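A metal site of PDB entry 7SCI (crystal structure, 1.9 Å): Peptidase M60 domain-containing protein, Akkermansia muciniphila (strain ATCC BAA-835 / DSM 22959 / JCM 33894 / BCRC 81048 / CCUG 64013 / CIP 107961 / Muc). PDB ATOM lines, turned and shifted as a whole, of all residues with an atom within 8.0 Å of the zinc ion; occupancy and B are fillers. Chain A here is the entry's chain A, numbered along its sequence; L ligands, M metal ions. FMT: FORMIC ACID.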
ATOM      1  N   ARG A 272      -2.619 -23.930 -32.307  1.00  0.00           N
ATOM      2  CA  ARG A 272      -1.774 -24.697 -31.407  1.00  0.00           C
ATOM      3  C   ARG A 272      -2.631 -25.516 -30.485  1.00  0.00           C
ATOM      4  O   ARG A 272      -3.662 -25.033 -29.999  1.00  0.00           O
ATOM      5  CB  ARG A 272      -0.855 -23.765 -30.605  1.00  0.00           C
ATOM      6  CG  ARG A 272       0.194 -24.495 -29.774  1.00  0.00           C
ATOM      7  CD  ARG A 272       0.844 -23.560 -28.749  1.00  0.00           C
ATOM      8  NE  ARG A 272      -0.127 -22.990 -27.845  1.00  0.00           N
ATOM      9  CZ  ARG A 272      -0.473 -23.518 -26.674  1.00  0.00           C
ATOM     10  NH1 ARG A 272       0.104 -24.653 -26.223  1.00  0.00           N
ATOM     11  NH2 ARG A 272      -1.395 -22.900 -25.964  1.00  0.00           N
ATOM     12  N   GLY A 303       3.124 -15.149 -35.715  1.00  0.00           N
ATOM     13  CA  GLY A 303       2.183 -16.225 -35.420  1.00  0.00           C
ATOM     14  C   GLY A 303       2.863 -17.383 -34.705  1.00  0.00           C
ATOM     15  O   GLY A 303       2.344 -17.879 -33.721  1.00  0.00           O
ATOM     16  N   HIS A 306       4.110 -16.102 -31.216  1.00  0.00           N
ATOM     17  CA  HIS A 306       2.928 -15.891 -30.344  1.00  0.00           C
ATOM     18  C   HIS A 306       2.465 -17.223 -29.739  1.00  0.00           C
ATOM     19  O   HIS A 306       2.167 -17.295 -28.549  1.00  0.00           O
ATOM     20  CB  HIS A 306       1.812 -15.256 -31.177  1.00  0.00           C
ATOM     21  CG  HIS A 306       0.533 -15.103 -30.429  1.00  0.00           C
ATOM     22  ND1 HIS A 306       0.205 -13.925 -29.767  1.00  0.00           N
ATOM     23  CD2 HIS A 306      -0.461 -15.976 -30.153  1.00  0.00           C
ATOM     24  CE1 HIS A 306      -0.962 -14.074 -29.166  1.00  0.00           C
ATOM     25  NE2 HIS A 306      -1.386 -15.306 -29.389  1.00  0.00           N
ATOM     26  N   GLU A 307       2.376 -18.259 -30.573  1.00  0.00           N
ATOM     27  CA  GLU A 307       1.890 -19.576 -30.139  1.00  0.00           C
ATOM     28  C   GLU A 307       2.850 -20.327 -29.254  1.00  0.00           C
ATOM     29  O   GLU A 307       2.470 -20.848 -28.211  1.00  0.00           O
ATOM     30  CB  GLU A 307       1.450 -20.445 -31.339  1.00  0.00           C
ATOM     31  CG  GLU A 307       0.143 -19.925 -31.972  1.00  0.00           C
ATOM     32  CD  GLU A 307      -1.107 -20.069 -31.078  1.00  0.00           C
ATOM     33  OE1 GLU A 307      -1.048 -20.390 -29.858  1.00  0.00           O
ATOM     34  OE2 GLU A 307      -2.186 -19.904 -31.653  1.00  0.00           O
ATOM     35  N   GLY A 309       5.029 -18.919 -27.573  1.00  0.00           N
ATOM     36  CA  GLY A 309       5.067 -18.085 -26.352  1.00  0.00           C
ATOM     37  C   GLY A 309       4.012 -18.466 -25.340  1.00  0.00           C
ATOM     38  O   GLY A 309       4.202 -18.223 -24.155  1.00  0.00           O
ATOM     39  N   HIS A 310       2.918 -19.079 -25.796  1.00  0.00           N
ATOM     40  CA  HIS A 310       1.954 -19.700 -24.856  1.00  0.00           C
ATOM     41  C   HIS A 310       2.516 -20.916 -24.120  1.00  0.00           C
ATOM     42  O   HIS A 310       2.165 -21.177 -22.981  1.00  0.00           O
ATOM     43  CB  HIS A 310       0.637 -20.074 -25.549  1.00  0.00           C
ATOM     44  CG  HIS A 310      -0.235 -18.896 -25.858  1.00  0.00           C
ATOM     45  ND1 HIS A 310      -0.637 -17.980 -24.901  1.00  0.00           N
ATOM     46  CD2 HIS A 310      -0.803 -18.504 -27.028  1.00  0.00           C
ATOM     47  CE1 HIS A 310      -1.414 -17.081 -25.471  1.00  0.00           C
ATOM     48  NE2 HIS A 310      -1.525 -17.366 -26.752  1.00  0.00           N
ATOM     49  N   GLN A 313       5.456 -18.894 -21.752  1.00  0.00           N
ATOM     50  CA  GLN A 313       5.118 -17.858 -20.767  1.00  0.00           C
ATOM     51  C   GLN A 313       5.025 -18.522 -19.374  1.00  0.00           C
ATOM     52  O   GLN A 313       4.421 -19.581 -19.223  1.00  0.00           O
ATOM     53  CB  GLN A 313       3.811 -17.110 -21.144  1.00  0.00           C
ATOM     54  CG  GLN A 313       2.537 -17.990 -21.150  1.00  0.00           C
ATOM     55  CD  GLN A 313       1.318 -17.331 -21.821  1.00  0.00           C
ATOM     56  OE1 GLN A 313       0.440 -18.026 -22.322  1.00  0.00           O
ATOM     57  NE2 GLN A 313       1.277 -15.999 -21.841  1.00  0.00           N
ATOM     58  N   THR A 323      -2.797 -13.826 -20.158  1.00  0.00           N
ATOM     59  CA  THR A 323      -2.572 -14.955 -21.109  1.00  0.00           C
ATOM     60  C   THR A 323      -2.165 -14.498 -22.511  1.00  0.00           C
ATOM     61  O   THR A 323      -1.289 -15.102 -23.136  1.00  0.00           O
ATOM     62  CB  THR A 323      -3.791 -15.908 -21.203  1.00  0.00           C
ATOM     63  OG1 THR A 323      -4.047 -16.397 -19.895  1.00  0.00           O
ATOM     64  CG2 THR A 323      -3.480 -17.106 -22.084  1.00  0.00           C
ATOM     65  N   GLU A 324      -2.800 -13.427 -22.987  1.00  0.00           N
ATOM     66  CA  GLU A 324      -2.534 -12.878 -24.324  1.00  0.00           C
ATOM     67  C   GLU A 324      -1.639 -11.636 -24.259  1.00  0.00           C
ATOM     68  O   GLU A 324      -1.542 -10.865 -25.229  1.00  0.00           O
ATOM     69  CB  GLU A 324      -3.848 -12.601 -25.069  1.00  0.00           C
ATOM     70  CG  GLU A 324      -4.746 -13.848 -25.225  1.00  0.00           C
ATOM     71  CD  GLU A 324      -4.146 -14.898 -26.147  1.00  0.00           C
ATOM     72  OE1 GLU A 324      -3.214 -14.599 -26.952  1.00  0.00           O
ATOM     73  OE2 GLU A 324      -4.583 -16.042 -26.095  1.00  0.00           O
ATOM     74  N   VAL A 325      -0.943 -11.480 -23.142  1.00  0.00           N
ATOM     75  CA  VAL A 325      -0.038 -10.367 -22.919  1.00  0.00           C
ATOM     76  C   VAL A 325       1.421 -10.880 -22.822  1.00  0.00           C
ATOM     77  O   VAL A 325       2.257 -10.546 -23.691  1.00  0.00           O
ATOM     78  CB  VAL A 325      -0.411  -9.574 -21.626  1.00  0.00           C
ATOM     79  CG1 VAL A 325       0.603  -8.437 -21.419  1.00  0.00           C
ATOM     80  CG2 VAL A 325      -1.852  -9.059 -21.695  1.00  0.00           C
ATOM     81  N   ASN A 327       3.024 -13.650 -23.443  1.00  0.00           N
ATOM     82  CA  ASN A 327       3.595 -14.392 -24.594  1.00  0.00           C
ATOM     83  C   ASN A 327       4.077 -13.448 -25.680  1.00  0.00           C
ATOM     84  O   ASN A 327       4.989 -13.776 -26.415  1.00  0.00           O
ATOM     85  CB  ASN A 327       2.571 -15.366 -25.195  1.00  0.00           C
ATOM     86  CG  ASN A 327       1.324 -14.675 -25.694  1.00  0.00           C
ATOM     87  OD1 ASN A 327       0.767 -13.780 -25.041  1.00  0.00           O
ATOM     88  ND2 ASN A 327       0.885 -15.061 -26.873  1.00  0.00           N
ATOM     89  N   ASN A 328       3.470 -12.264 -25.778  1.00  0.00           N
ATOM     90  CA  ASN A 328       3.875 -11.331 -26.834  1.00  0.00           C
ATOM     91  C   ASN A 328       5.134 -10.560 -26.529  1.00  0.00           C
ATOM     92  O   ASN A 328       5.660  -9.885 -27.405  1.00  0.00           O
ATOM     93  CB  ASN A 328       2.712 -10.397 -27.232  1.00  0.00           C
ATOM     94  CG  ASN A 328       1.772 -11.039 -28.240  1.00  0.00           C
ATOM     95  OD1 ASN A 328       2.124 -11.991 -28.963  1.00  0.00           O
ATOM     96  ND2 ASN A 328       0.548 -10.487 -28.319  1.00  0.00           N
ATOM     97  N   TYR A 451      -9.529 -16.014 -20.635  1.00  0.00           N
ATOM     98  CA  TYR A 451     -10.237 -17.264 -20.955  1.00  0.00           C
ATOM     99  C   TYR A 451     -11.029 -17.746 -19.727  1.00  0.00           C
ATOM    100  O   TYR A 451     -12.120 -18.320 -19.843  1.00  0.00           O
ATOM    101  CB  TYR A 451      -9.235 -18.305 -21.458  1.00  0.00           C
ATOM    102  CG  TYR A 451      -8.631 -17.851 -22.752  1.00  0.00           C
ATOM    103  CD1 TYR A 451      -9.406 -17.853 -23.950  1.00  0.00           C
ATOM    104  CD2 TYR A 451      -7.308 -17.349 -22.806  1.00  0.00           C
ATOM    105  CE1 TYR A 451      -8.870 -17.401 -25.144  1.00  0.00           C
ATOM    106  CE2 TYR A 451      -6.752 -16.893 -24.013  1.00  0.00           C
ATOM    107  CZ  TYR A 451      -7.546 -16.923 -25.165  1.00  0.00           C
ATOM    108  OH  TYR A 451      -7.047 -16.476 -26.364  1.00  0.00           O
HETATM  109  C   FMT L   1      -4.334 -17.921 -30.363  1.00  0.00           C
HETATM  110  O1  FMT L   1      -3.723 -17.747 -29.320  1.00  0.00           O
HETATM  111  O2  FMT L   1      -5.652 -18.028 -30.298  1.00  0.00           O
HETATM  112 ZN    ZN M   1      -2.756 -16.229 -28.070  1.00  0.00          ZN
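Of the 13 residues printed, 3 come within 4 Å of the zinc ion.
The nearest printed residue that does not touch the zinc ion is Asn 327 (4.01 Å).
OH of Tyr 451 sits at hydrogen-bond distance from OE2 of Glu 324 (2.5 Å).
The backbone carbonyl oxygen (O) of His 306 lies within hydrogen-bond range of the side-chain amide nitrogen (ND2) of Asn 327 (3.1 Å).
OD1 of Asn 328 sits at hydrogen-bond distance from ND1 of His 306, at 2.8 Å.
NE2 of His 310 lies close to ND2 of Asn 327 (3.3 Å).
A ring nitrogen (ND1) of His 310 lies close to the backbone carbonyl oxygen (O) of Thr 323 (3.4 Å).
A ring nitrogen (ND1) of His 310 sits at hydrogen-bond distance from the side-chain amide oxygen (OE1) of Gln 313, 2.8 Å away.
The zinc ion is bound by the side-chain carboxylate (OE1) of Glu 324 (2.0 Å), a ring nitrogen (NE2) of His 306 (2.1 Å), a ring nitrogen (NE2) of His 310 (2.1 Å) and an oxygen (O1) of the ligand (2.2 Å).
The zinc ion has four donor atoms within binding distance.
Slightly farther from the zinc ion lies OE2 of Glu 324 (2.7 Å).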
